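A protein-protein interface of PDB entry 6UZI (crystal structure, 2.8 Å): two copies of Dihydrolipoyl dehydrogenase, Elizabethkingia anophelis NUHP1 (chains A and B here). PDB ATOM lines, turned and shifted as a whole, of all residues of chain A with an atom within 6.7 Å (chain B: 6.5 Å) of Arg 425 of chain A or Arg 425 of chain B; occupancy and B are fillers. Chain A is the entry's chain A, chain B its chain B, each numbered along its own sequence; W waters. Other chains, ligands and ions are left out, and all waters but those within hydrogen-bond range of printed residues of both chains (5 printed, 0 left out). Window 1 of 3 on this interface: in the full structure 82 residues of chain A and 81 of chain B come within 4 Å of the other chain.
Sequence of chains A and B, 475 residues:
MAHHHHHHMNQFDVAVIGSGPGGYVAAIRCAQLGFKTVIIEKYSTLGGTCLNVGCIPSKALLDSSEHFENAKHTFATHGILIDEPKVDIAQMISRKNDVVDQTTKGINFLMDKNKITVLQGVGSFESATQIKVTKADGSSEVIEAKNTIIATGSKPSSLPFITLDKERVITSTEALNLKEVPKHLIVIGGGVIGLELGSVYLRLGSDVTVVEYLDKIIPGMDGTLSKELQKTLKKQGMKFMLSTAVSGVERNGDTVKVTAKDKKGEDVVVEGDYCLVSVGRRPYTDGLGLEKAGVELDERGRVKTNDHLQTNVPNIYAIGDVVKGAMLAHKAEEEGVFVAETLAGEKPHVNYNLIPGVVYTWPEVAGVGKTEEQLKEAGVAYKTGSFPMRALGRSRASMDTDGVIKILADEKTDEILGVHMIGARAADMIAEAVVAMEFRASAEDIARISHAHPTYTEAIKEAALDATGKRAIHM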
ATOM      1  N   ASP A  63      14.849 -34.776 -31.224  1.00  0.00           N
ATOM      2  CA  ASP A  63      13.465 -34.986 -30.821  1.00  0.00           C
ATOM      3  C   ASP A  63      13.022 -36.415 -31.099  1.00  0.00           C
ATOM      4  O   ASP A  63      12.342 -37.035 -30.272  1.00  0.00           O
ATOM      5  CB  ASP A  63      12.558 -33.988 -31.536  1.00  0.00           C
ATOM      6  CG  ASP A  63      12.741 -32.574 -31.027  1.00  0.00           C
ATOM      7  OD1 ASP A  63      12.408 -31.625 -31.770  1.00  0.00           O
ATOM      8  OD2 ASP A  63      13.235 -32.409 -29.890  1.00  0.00           O
ATOM      9  N   TRP A 362      19.314 -33.726 -23.444  1.00  0.00           N
ATOM     10  CA  TRP A 362      18.210 -33.919 -22.503  1.00  0.00           C
ATOM     11  C   TRP A 362      18.742 -34.515 -21.208  1.00  0.00           C
ATOM     12  O   TRP A 362      19.130 -35.703 -21.190  1.00  0.00           O
ATOM     13  CB  TRP A 362      17.108 -34.796 -23.088  1.00  0.00           C
ATOM     14  CG  TRP A 362      15.833 -34.725 -22.285  1.00  0.00           C
ATOM     15  CD1 TRP A 362      15.316 -35.701 -21.483  1.00  0.00           C
ATOM     16  CD2 TRP A 362      14.936 -33.611 -22.189  1.00  0.00           C
ATOM     17  NE1 TRP A 362      14.150 -35.272 -20.905  1.00  0.00           N
ATOM     18  CE2 TRP A 362      13.894 -33.990 -21.318  1.00  0.00           C
ATOM     19  CE3 TRP A 362      14.908 -32.333 -22.759  1.00  0.00           C
ATOM     20  CZ2 TRP A 362      12.834 -33.140 -21.003  1.00  0.00           C
ATOM     21  CZ3 TRP A 362      13.855 -31.489 -22.446  1.00  0.00           C
ATOM     22  CH2 TRP A 362      12.832 -31.897 -21.573  1.00  0.00           C
ATOM     23  N   PRO A 363      18.742 -33.762 -20.095  1.00  0.00           N
ATOM     24  CA  PRO A 363      18.168 -32.416 -19.935  1.00  0.00           C
ATOM     25  C   PRO A 363      18.859 -31.341 -20.757  1.00  0.00           C
ATOM     26  O   PRO A 363      20.028 -31.481 -21.109  1.00  0.00           O
ATOM     27  CB  PRO A 363      18.359 -32.137 -18.443  1.00  0.00           C
ATOM     28  CG  PRO A 363      19.560 -32.926 -18.083  1.00  0.00           C
ATOM     29  CD  PRO A 363      19.430 -34.199 -18.870  1.00  0.00           C
ATOM     30  N   GLU A 364      18.126 -30.287 -21.086  1.00  0.00           N
ATOM     31  CA  GLU A 364      18.722 -29.158 -21.782  1.00  0.00           C
ATOM     32  C   GLU A 364      19.615 -28.359 -20.836  1.00  0.00           C
ATOM     33  O   GLU A 364      19.429 -28.357 -19.616  1.00  0.00           O
ATOM     34  CB  GLU A 364      17.630 -28.271 -22.369  1.00  0.00           C
ATOM     35  CG  GLU A 364      16.969 -28.851 -23.616  1.00  0.00           C
ATOM     36  CD  GLU A 364      15.603 -28.235 -23.911  1.00  0.00           C
ATOM     37  OE1 GLU A 364      15.148 -27.354 -23.138  1.00  0.00           O
ATOM     38  OE2 GLU A 364      14.988 -28.631 -24.926  1.00  0.00           O
ATOM     39  N   MET A 389      16.445 -29.901  -9.561  1.00  0.00           N
ATOM     40  CA  MET A 389      15.271 -30.168 -10.389  1.00  0.00           C
ATOM     41  C   MET A 389      14.448 -31.335  -9.862  1.00  0.00           C
ATOM     42  O   MET A 389      13.229 -31.371 -10.062  1.00  0.00           O
ATOM     43  CB  MET A 389      15.685 -30.449 -11.834  1.00  0.00           C
ATOM     44  CG  MET A 389      16.305 -29.275 -12.566  1.00  0.00           C
ATOM     45  SD  MET A 389      15.154 -27.916 -12.792  1.00  0.00           S
ATOM     46  CE  MET A 389      13.970 -28.644 -13.916  1.00  0.00           C
ATOM     47  N   ARG A 394       6.610 -30.964 -10.672  1.00  0.00           N
ATOM     48  CA  ARG A 394       6.502 -31.158 -12.114  1.00  0.00           C
ATOM     49  C   ARG A 394       7.477 -32.224 -12.607  1.00  0.00           C
ATOM     50  O   ARG A 394       7.114 -33.069 -13.435  1.00  0.00           O
ATOM     51  CB  ARG A 394       6.737 -29.831 -12.836  1.00  0.00           C
ATOM     52  CG  ARG A 394       6.403 -29.869 -14.312  1.00  0.00           C
ATOM     53  CD  ARG A 394       4.918 -30.108 -14.510  1.00  0.00           C
ATOM     54  NE  ARG A 394       4.565 -30.370 -15.902  1.00  0.00           N
ATOM     55  CZ  ARG A 394       4.427 -31.587 -16.419  1.00  0.00           C
ATOM     56  NH1 ARG A 394       4.619 -32.657 -15.659  1.00  0.00           N
ATOM     57  NH2 ARG A 394       4.096 -31.736 -17.693  1.00  0.00           N
ATOM     58  N   MET A 421      21.524 -23.123 -15.931  1.00  0.00           N
ATOM     59  CA  MET A 421      20.482 -24.129 -15.810  1.00  0.00           C
ATOM     60  C   MET A 421      20.895 -25.421 -16.490  1.00  0.00           C
ATOM     61  O   MET A 421      21.513 -25.410 -17.560  1.00  0.00           O
ATOM     62  CB  MET A 421      19.168 -23.656 -16.446  1.00  0.00           C
ATOM     63  CG  MET A 421      18.773 -22.230 -16.163  1.00  0.00           C
ATOM     64  SD  MET A 421      17.194 -21.903 -16.975  1.00  0.00           S
ATOM     65  CE  MET A 421      16.830 -20.264 -16.344  1.00  0.00           C
ATOM     66  N   GLY A 423      18.371 -28.922 -16.933  1.00  0.00           N
ATOM     67  CA  GLY A 423      17.112 -29.511 -16.531  1.00  0.00           C
ATOM     68  C   GLY A 423      16.153 -29.523 -17.696  1.00  0.00           C
ATOM     69  O   GLY A 423      16.470 -29.057 -18.793  1.00  0.00           O
ATOM     70  N   ALA A 424      14.965 -30.067 -17.434  1.00  0.00           N
ATOM     71  CA  ALA A 424      13.939 -30.138 -18.468  1.00  0.00           C
ATOM     72  C   ALA A 424      13.556 -28.739 -18.927  1.00  0.00           C
ATOM     73  O   ALA A 424      13.388 -27.829 -18.114  1.00  0.00           O
ATOM     74  CB  ALA A 424      12.703 -30.871 -17.946  1.00  0.00           C
ATOM     75  N   ARG A 425      13.436 -28.575 -20.245  1.00  0.00           N
ATOM     76  CA  ARG A 425      12.981 -27.341 -20.886  1.00  0.00           C
ATOM     77  C   ARG A 425      13.881 -26.141 -20.586  1.00  0.00           C
ATOM     78  O   ARG A 425      13.436 -24.990 -20.678  1.00  0.00           O
ATOM     79  CB  ARG A 425      11.536 -27.011 -20.494  1.00  0.00           C
ATOM     80  CG  ARG A 425      10.545 -28.099 -20.786  1.00  0.00           C
ATOM     81  CD  ARG A 425       9.137 -27.655 -20.424  1.00  0.00           C
ATOM     82  NE  ARG A 425       8.148 -28.638 -20.848  1.00  0.00           N
ATOM     83  CZ  ARG A 425       6.844 -28.400 -20.917  1.00  0.00           C
ATOM     84  NH1 ARG A 425       6.375 -27.198 -20.608  1.00  0.00           N
ATOM     85  NH2 ARG A 425       6.015 -29.356 -21.330  1.00  0.00           N
ATOM     86  N   ALA A 426      15.145 -26.374 -20.231  1.00  0.00           N
ATOM     87  CA  ALA A 426      16.032 -25.254 -19.928  1.00  0.00           C
ATOM     88  C   ALA A 426      16.228 -24.348 -21.133  1.00  0.00           C
ATOM     89  O   ALA A 426      16.488 -23.151 -20.972  1.00  0.00           O
ATOM     90  CB  ALA A 426      17.380 -25.760 -19.421  1.00  0.00           C
ATOM     91  N   ALA A 427      16.131 -24.903 -22.345  1.00  0.00           N
ATOM     92  CA  ALA A 427      16.325 -24.085 -23.536  1.00  0.00           C
ATOM     93  C   ALA A 427      15.313 -22.947 -23.606  1.00  0.00           C
ATOM     94  O   ALA A 427      15.599 -21.901 -24.192  1.00  0.00           O
ATOM     95  CB  ALA A 427      16.249 -24.955 -24.791  1.00  0.00           C
ATOM     96  N   ASP A 428      14.136 -23.119 -23.008  1.00  0.00           N
ATOM     97  CA  ASP A 428      13.144 -22.057 -22.978  1.00  0.00           C
ATOM     98  C   ASP A 428      13.004 -21.396 -21.615  1.00  0.00           C
ATOM     99  O   ASP A 428      12.590 -20.238 -21.551  1.00  0.00           O
ATOM    100  CB  ASP A 428      11.779 -22.590 -23.435  1.00  0.00           C
ATOM    101  CG  ASP A 428      11.804 -23.081 -24.870  1.00  0.00           C
ATOM    102  OD1 ASP A 428      11.866 -24.309 -25.088  1.00  0.00           O
ATOM    103  OD2 ASP A 428      11.777 -22.239 -25.787  1.00  0.00           O
ATOM    104  N   MET A 429      13.372 -22.078 -20.532  1.00  0.00           N
ATOM    105  CA  MET A 429      13.352 -21.425 -19.230  1.00  0.00           C
ATOM    106  C   MET A 429      14.362 -20.287 -19.174  1.00  0.00           C
ATOM    107  O   MET A 429      14.166 -19.312 -18.438  1.00  0.00           O
ATOM    108  CB  MET A 429      13.650 -22.433 -18.126  1.00  0.00           C
ATOM    109  CG  MET A 429      12.546 -23.413 -17.855  1.00  0.00           C
ATOM    110  SD  MET A 429      12.816 -24.211 -16.271  1.00  0.00           S
ATOM    111  CE  MET A 429      14.367 -25.058 -16.541  1.00  0.00           C
ATOM    112  N   ILE A 430      15.444 -20.397 -19.946  1.00  0.00           N
ATOM    113  CA  ILE A 430      16.520 -19.420 -19.888  1.00  0.00           C
ATOM    114  C   ILE A 430      16.031 -18.029 -20.265  1.00  0.00           C
ATOM    115  O   ILE A 430      16.625 -17.030 -19.844  1.00  0.00           O
ATOM    116  CB  ILE A 430      17.684 -19.886 -20.789  1.00  0.00           C
ATOM    117  CG1 ILE A 430      18.954 -19.108 -20.470  1.00  0.00           C
ATOM    118  CG2 ILE A 430      17.333 -19.735 -22.264  1.00  0.00           C
ATOM    119  CD1 ILE A 430      19.411 -19.294 -19.060  1.00  0.00           C
ATOM    120  N   TYR A 456       8.547 -26.154 -14.372  1.00  0.00           N
ATOM    121  CA  TYR A 456       9.981 -26.262 -14.138  1.00  0.00           C
ATOM    122  C   TYR A 456      10.577 -24.925 -13.723  1.00  0.00           C
ATOM    123  O   TYR A 456      11.605 -24.894 -13.037  1.00  0.00           O
ATOM    124  CB  TYR A 456      10.675 -26.799 -15.386  1.00  0.00           C
ATOM    125  CG  TYR A 456      10.203 -28.178 -15.765  1.00  0.00           C
ATOM    126  CD1 TYR A 456       9.452 -28.385 -16.920  1.00  0.00           C
ATOM    127  CD2 TYR A 456      10.465 -29.270 -14.943  1.00  0.00           C
ATOM    128  CE1 TYR A 456       9.000 -29.644 -17.261  1.00  0.00           C
ATOM    129  CE2 TYR A 456      10.018 -30.538 -15.279  1.00  0.00           C
ATOM    130  CZ  TYR A 456       9.286 -30.718 -16.439  1.00  0.00           C
ATOM    131  OH  TYR A 456       8.837 -31.973 -16.771  1.00  0.00           O
ATOM    132  N   ASP B  63       1.134 -36.509 -18.760  1.00  0.00           N
ATOM    133  CA  ASP B  63       2.420 -36.904 -19.319  1.00  0.00           C
ATOM    134  C   ASP B  63       2.368 -38.322 -19.869  1.00  0.00           C
ATOM    135  O   ASP B  63       2.903 -38.597 -20.950  1.00  0.00           O
ATOM    136  CB  ASP B  63       3.498 -36.785 -18.243  1.00  0.00           C
ATOM    137  CG  ASP B  63       3.789 -35.350 -17.875  1.00  0.00           C
ATOM    138  OD1 ASP B  63       3.495 -34.454 -18.693  1.00  0.00           O
ATOM    139  OD2 ASP B  63       4.292 -35.115 -16.757  1.00  0.00           O
ATOM    140  N   TRP B 362      -1.877 -30.328 -24.513  1.00  0.00           N
ATOM    141  CA  TRP B 362      -0.774 -30.287 -25.471  1.00  0.00           C
ATOM    142  C   TRP B 362      -1.318 -29.916 -26.841  1.00  0.00           C
ATOM    143  O   TRP B 362      -1.973 -30.758 -27.488  1.00  0.00           O
ATOM    144  CB  TRP B 362      -0.008 -31.604 -25.524  1.00  0.00           C
ATOM    145  CG  TRP B 362       1.317 -31.426 -26.202  1.00  0.00           C
ATOM    146  CD1 TRP B 362       1.675 -31.880 -27.437  1.00  0.00           C
ATOM    147  CD2 TRP B 362       2.443 -30.697 -25.701  1.00  0.00           C
ATOM    148  NE1 TRP B 362       2.956 -31.495 -27.727  1.00  0.00           N
ATOM    149  CE2 TRP B 362       3.455 -30.774 -26.674  1.00  0.00           C
ATOM    150  CE3 TRP B 362       2.695 -29.993 -24.519  1.00  0.00           C
ATOM    151  CZ2 TRP B 362       4.700 -30.176 -26.505  1.00  0.00           C
ATOM    152  CZ3 TRP B 362       3.937 -29.402 -24.351  1.00  0.00           C
ATOM    153  CH2 TRP B 362       4.922 -29.496 -25.342  1.00  0.00           C
ATOM    154  N   PRO B 363      -1.031 -28.705 -27.352  1.00  0.00           N
ATOM    155  CA  PRO B 363      -0.138 -27.691 -26.775  1.00  0.00           C
ATOM    156  C   PRO B 363      -0.616 -27.108 -25.451  1.00  0.00           C
ATOM    157  O   PRO B 363      -1.814 -27.086 -25.190  1.00  0.00           O
ATOM    158  CB  PRO B 363      -0.124 -26.598 -27.849  1.00  0.00           C
ATOM    159  CG  PRO B 363      -1.432 -26.728 -28.520  1.00  0.00           C
ATOM    160  CD  PRO B 363      -1.678 -28.213 -28.580  1.00  0.00           C
ATOM    161  N   GLU B 364       0.323 -26.655 -24.627  1.00  0.00           N
ATOM    162  CA  GLU B 364      -0.024 -25.984 -23.385  1.00  0.00           C
ATOM    163  C   GLU B 364      -0.576 -24.588 -23.666  1.00  0.00           C
ATOM    164  O   GLU B 364      -0.299 -23.975 -24.703  1.00  0.00           O
ATOM    165  CB  GLU B 364       1.196 -25.905 -22.466  1.00  0.00           C
ATOM    166  CG  GLU B 364       1.524 -27.225 -21.763  1.00  0.00           C
ATOM    167  CD  GLU B 364       2.955 -27.303 -21.236  1.00  0.00           C
ATOM    168  OE1 GLU B 364       3.729 -26.340 -21.429  1.00  0.00           O
ATOM    169  OE2 GLU B 364       3.298 -28.332 -20.610  1.00  0.00           O
ATOM    170  N   MET B 389       2.989 -20.495 -34.051  1.00  0.00           N
ATOM    171  CA  MET B 389       4.021 -21.455 -33.659  1.00  0.00           C
ATOM    172  C   MET B 389       4.510 -22.289 -34.841  1.00  0.00           C
ATOM    173  O   MET B 389       5.684 -22.681 -34.874  1.00  0.00           O
ATOM    174  CB  MET B 389       3.493 -22.377 -32.557  1.00  0.00           C
ATOM    175  CG  MET B 389       3.178 -21.682 -31.233  1.00  0.00           C
ATOM    176  SD  MET B 389       4.608 -21.004 -30.364  1.00  0.00           S
ATOM    177  CE  MET B 389       5.481 -22.484 -29.881  1.00  0.00           C
ATOM    178  N   ARG B 394      11.976 -24.578 -34.521  1.00  0.00           N
ATOM    179  CA  ARG B 394      11.917 -25.533 -33.418  1.00  0.00           C
ATOM    180  C   ARG B 394      10.634 -26.360 -33.461  1.00  0.00           C
ATOM    181  O   ARG B 394      10.657 -27.570 -33.199  1.00  0.00           O
ATOM    182  CB  ARG B 394      12.042 -24.796 -32.082  1.00  0.00           C
ATOM    183  CG  ARG B 394      12.247 -25.718 -30.886  1.00  0.00           C
ATOM    184  CD  ARG B 394      13.568 -26.445 -31.018  1.00  0.00           C
ATOM    185  NE  ARG B 394      13.762 -27.514 -30.043  1.00  0.00           N
ATOM    186  CZ  ARG B 394      13.475 -28.794 -30.269  1.00  0.00           C
ATOM    187  NH1 ARG B 394      12.965 -29.164 -31.437  1.00  0.00           N
ATOM    188  NH2 ARG B 394      13.704 -29.706 -29.331  1.00  0.00           N
ATOM    189  N   MET B 421      -0.602 -17.248 -24.636  1.00  0.00           N
ATOM    190  CA  MET B 421       0.140 -18.267 -25.361  1.00  0.00           C
ATOM    191  C   MET B 421      -0.653 -19.559 -25.473  1.00  0.00           C
ATOM    192  O   MET B 421      -1.285 -20.005 -24.510  1.00  0.00           O
ATOM    193  CB  MET B 421       1.465 -18.581 -24.663  1.00  0.00           C
ATOM    194  CG  MET B 421       2.241 -17.377 -24.202  1.00  0.00           C
ATOM    195  SD  MET B 421       3.767 -17.935 -23.434  1.00  0.00           S
ATOM    196  CE  MET B 421       4.638 -16.388 -23.210  1.00  0.00           C
ATOM    197  N   GLY B 423       0.811 -23.219 -27.240  1.00  0.00           N
ATOM    198  CA  GLY B 423       1.926 -23.782 -27.974  1.00  0.00           C
ATOM    199  C   GLY B 423       2.741 -24.686 -27.074  1.00  0.00           C
ATOM    200  O   GLY B 423       2.430 -24.879 -25.896  1.00  0.00           O
ATOM    201  N   ALA B 424       3.783 -25.262 -27.662  1.00  0.00           N
ATOM    202  CA  ALA B 424       4.651 -26.144 -26.896  1.00  0.00           C
ATOM    203  C   ALA B 424       5.318 -25.370 -25.767  1.00  0.00           C
ATOM    204  O   ALA B 424       5.720 -24.218 -25.937  1.00  0.00           O
ATOM    205  CB  ALA B 424       5.710 -26.782 -27.802  1.00  0.00           C
ATOM    206  N   ARG B 425       5.384 -25.992 -24.592  1.00  0.00           N
ATOM    207  CA  ARG B 425       6.104 -25.457 -23.437  1.00  0.00           C
ATOM    208  C   ARG B 425       5.564 -24.106 -22.968  1.00  0.00           C
ATOM    209  O   ARG B 425       6.279 -23.337 -22.312  1.00  0.00           O
ATOM    210  CB  ARG B 425       7.607 -25.350 -23.726  1.00  0.00           C
ATOM    211  CG  ARG B 425       8.246 -26.656 -24.128  1.00  0.00           C
ATOM    212  CD  ARG B 425       9.735 -26.486 -24.317  1.00  0.00           C
ATOM    213  NE  ARG B 425      10.409 -27.762 -24.528  1.00  0.00           N
ATOM    214  CZ  ARG B 425      11.726 -27.924 -24.478  1.00  0.00           C
ATOM    215  NH1 ARG B 425      12.252 -29.119 -24.679  1.00  0.00           N
ATOM    216  NH2 ARG B 425      12.512 -26.893 -24.210  1.00  0.00           N
ATOM    217  N   ALA B 426       4.305 -23.802 -23.280  1.00  0.00           N
ATOM    218  CA  ALA B 426       3.733 -22.540 -22.837  1.00  0.00           C
ATOM    219  C   ALA B 426       3.724 -22.443 -21.320  1.00  0.00           C
ATOM    220  O   ALA B 426       3.876 -21.348 -20.765  1.00  0.00           O
ATOM    221  CB  ALA B 426       2.317 -22.386 -23.389  1.00  0.00           C
ATOM    222  N   ALA B 427       3.599 -23.582 -20.633  1.00  0.00           N
ATOM    223  CA  ALA B 427       3.557 -23.564 -19.175  1.00  0.00           C
ATOM    224  C   ALA B 427       4.816 -22.952 -18.585  1.00  0.00           C
ATOM    225  O   ALA B 427       4.768 -22.371 -17.497  1.00  0.00           O
ATOM    226  CB  ALA B 427       3.358 -24.978 -18.634  1.00  0.00           C
ATOM    227  N   ASP B 428       5.942 -23.043 -19.293  1.00  0.00           N
ATOM    228  CA  ASP B 428       7.177 -22.449 -18.814  1.00  0.00           C
ATOM    229  C   ASP B 428       7.578 -21.184 -19.555  1.00  0.00           C
ATOM    230  O   ASP B 428       8.302 -20.364 -18.986  1.00  0.00           O
ATOM    231  CB  ASP B 428       8.324 -23.468 -18.890  1.00  0.00           C
ATOM    232  CG  ASP B 428       8.101 -24.651 -17.976  1.00  0.00           C
ATOM    233  OD1 ASP B 428       7.644 -25.703 -18.472  1.00  0.00           O
ATOM    234  OD2 ASP B 428       8.343 -24.513 -16.754  1.00  0.00           O
ATOM    235  N   MET B 429       7.122 -20.997 -20.793  1.00  0.00           N
ATOM    236  CA  MET B 429       7.403 -19.746 -21.485  1.00  0.00           C
ATOM    237  C   MET B 429       6.709 -18.568 -20.815  1.00  0.00           C
ATOM    238  O   MET B 429       7.213 -17.438 -20.875  1.00  0.00           O
ATOM    239  CB  MET B 429       6.970 -19.832 -22.943  1.00  0.00           C
ATOM    240  CG  MET B 429       7.855 -20.693 -23.819  1.00  0.00           C
ATOM    241  SD  MET B 429       7.518 -20.360 -25.558  1.00  0.00           S
ATOM    242  CE  MET B 429       5.798 -20.851 -25.683  1.00  0.00           C
ATOM    243  N   ILE B 430       5.563 -18.808 -20.171  1.00  0.00           N
ATOM    244  CA  ILE B 430       4.801 -17.707 -19.596  1.00  0.00           C
ATOM    245  C   ILE B 430       5.632 -16.965 -18.560  1.00  0.00           C
ATOM    246  O   ILE B 430       5.402 -15.776 -18.315  1.00  0.00           O
ATOM    247  CB  ILE B 430       3.467 -18.220 -18.999  1.00  0.00           C
ATOM    248  CG1 ILE B 430       2.498 -17.057 -18.774  1.00  0.00           C
ATOM    249  CG2 ILE B 430       3.694 -18.970 -17.686  1.00  0.00           C
ATOM    250  CD1 ILE B 430       2.130 -16.329 -20.041  1.00  0.00           C
ATOM    251  N   TYR B 456      11.254 -22.117 -28.627  1.00  0.00           N
ATOM    252  CA  TYR B 456       9.868 -21.692 -28.751  1.00  0.00           C
ATOM    253  C   TYR B 456       9.689 -20.244 -28.306  1.00  0.00           C
ATOM    254  O   TYR B 456       8.774 -19.562 -28.781  1.00  0.00           O
ATOM    255  CB  TYR B 456       8.964 -22.628 -27.950  1.00  0.00           C
ATOM    256  CG  TYR B 456       9.017 -24.067 -28.415  1.00  0.00           C
ATOM    257  CD1 TYR B 456       8.571 -24.427 -29.682  1.00  0.00           C
ATOM    258  CD2 TYR B 456       9.498 -25.068 -27.585  1.00  0.00           C
ATOM    259  CE1 TYR B 456       8.615 -25.746 -30.112  1.00  0.00           C
ATOM    260  CE2 TYR B 456       9.538 -26.386 -28.002  1.00  0.00           C
ATOM    261  CZ  TYR B 456       9.097 -26.720 -29.267  1.00  0.00           C
ATOM    262  OH  TYR B 456       9.143 -28.033 -29.685  1.00  0.00           O
HETATM  263  O   HOH W   1       1.955 -31.142 -20.136  1.00  0.00           O
HETATM  264  O   HOH W   2      15.721 -30.640 -26.774  1.00  0.00           O
HETATM  265  O   HOH W   3       5.881 -33.807 -19.684  1.00  0.00           O
HETATM  266  O   HOH W   4      14.728 -27.259 -27.190  1.00  0.00           O
HETATM  267  O   HOH W   5       6.505 -27.297 -16.649  1.00  0.00           O
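Water W4 lies within hydrogen-bond range of the side-chain carboxylate of Glu 364 of chain A and the guanidinium group of Arg 394 of chain B. Water W3 bridges the side-chain carboxylate (OD1) of Asp 63 of chain B (2.7 Å) and the guanidinium group (NH2) of Arg 394 of chain A (3.4 Å). Water W5 bridges the side-chain carboxylate of Asp 428 of chain B (2.7 Å) and the backbone NH of Tyr 456 of chain A (3.3 Å). Water W2 bridges OE2 of Glu 364 of chain A (2.8 Å) and NH2 of Arg 394 of chain B (3.4 Å). Water W1 bridges the side-chain carboxylate of Glu 364 of chain B (3.2 Å) and the guanidinium group of Arg 394 of chain A (3.3 Å).
Of the 16 printed residues of chain A, 7 touch a printed residue of chain B. Of the 16 printed residues of chain B, 7 touch a printed residue of chain A. Along chain B the printed residues that touch a printed residue of chain A span positions 63 to 456.
Among the printed residues, pairs that only touch across the chains: Trp 362 of chain A with Arg 425 of chain B (3.6 Å), Arg 425 of chain A with Trp 362 of chain B (3.7 Å) and Arg 425 of chain A with Arg 425 of chain B (3.3 Å).
Of chain B, only Trp 362 (3.7 Å), Glu 364 (2.9 Å), Arg 425 (3.3 Å) and Asp 428 (2.9 Å) come within 4 Å of Arg 425 of chain A. Arg 425 of chain B touches four residues of chain A. Of the printed residues of chain A, Asp 428 of chain B touches Arg 425 (2.9 Å) and Tyr 456 (2.9 Å). Of the printed residues of chain B, Asp 63 of chain A touches Arg 394 (2.5 Å). Of the printed residues of chain B, Asp 428 of chain A touches Arg 425 and Tyr 456. Printed residues of chain B within 4 Å of Trp 362 of chain A: Arg 425. Ile 430 of chain A touches none of the printed residues of chain B. Met 421 of chain A touches none of the printed residues of chain B.
The backbone carbonyl oxygen (O) of Glu 364 of chain B is in hydrogen-bond range of the backbone NH (N) of Gly 423 of chain B, 2.9 Å away. N of Ala 427 of chain A lies within hydrogen-bond range of OE1 of Glu 364 of chain A, at 2.8 Å. N of Ala 427 of chain B is in hydrogen-bond range of OE1 of Glu 364 of chain B (2.9 Å). The side-chain carboxylate (OE1) of Glu 364 of chain B lies within hydrogen-bond range of the backbone NH (N) of Ala 426 of chain B, at 3.2 Å. The side-chain carboxylate (OE1) of Glu 364 of chain A lies within hydrogen-bond range of the backbone NH (N) of Ala 426 of chain A, 3.1 Å away. The backbone carbonyl oxygen (O) of Glu 364 of chain A sits at hydrogen-bond distance from the backbone NH (N) of Gly 423 of chain A, 2.9 Å away.
Asp 63 of chain A touches Arg 394 of chain B, and with the chains exchanged Arg 394 of chain A touches Asp 63 of chain B. Trp 362 of chain A touches Arg 425 of chain B, and with the chains exchanged Arg 425 of chain A touches Trp 362 of chain B. Arg 425 of chain A touches Asp 428 of chain B, and with the chains exchanged Asp 428 of chain A touches Arg 425 of chain B. Asp 428 of chain A touches Tyr 456 of chain B, and with the chains exchanged Tyr 456 of chain A touches Asp 428 of chain B. Positions printed for both chains: 63, 362, 363, 364, 389, 394, 421, 423, 424, 425, 426, 427, 428, 429, 430 and 456.
OD2 of Asp 428 of chain A lies within hydrogen-bond range of N of Tyr 456 of chain B, 2.9 Å away. The side-chain carboxylate (OD2) of Asp 63 of chain B lies within salt-bridge range of the guanidinium group (NH1) of Arg 394 of chain A (2.7 Å). The guanidinium group (NH2) of Arg 425 of chain B is in salt-bridge range of the side-chain carboxylate (OD1) of Asp 428 of chain A, 2.8 Å away. The side-chain carboxylate of Asp 63 of chain A lies within salt-bridge range of the guanidinium group of Arg 394 of chain B (2.5 Å). OE1 of Glu 364 of chain B is in salt-bridge range of NH1 of Arg 425 of chain A (2.9 Å). N of Tyr 456 of chain A sits at hydrogen-bond distance from OD2 of Asp 428 of chain B, 2.9 Å away. NH1 of Arg 425 of chain A lies within salt-bridge range of OD1 of Asp 428 of chain B. NH1 of Arg 425 of chain B lies within salt-bridge range of OE2 of Glu 364 of chain A (2.8 Å).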
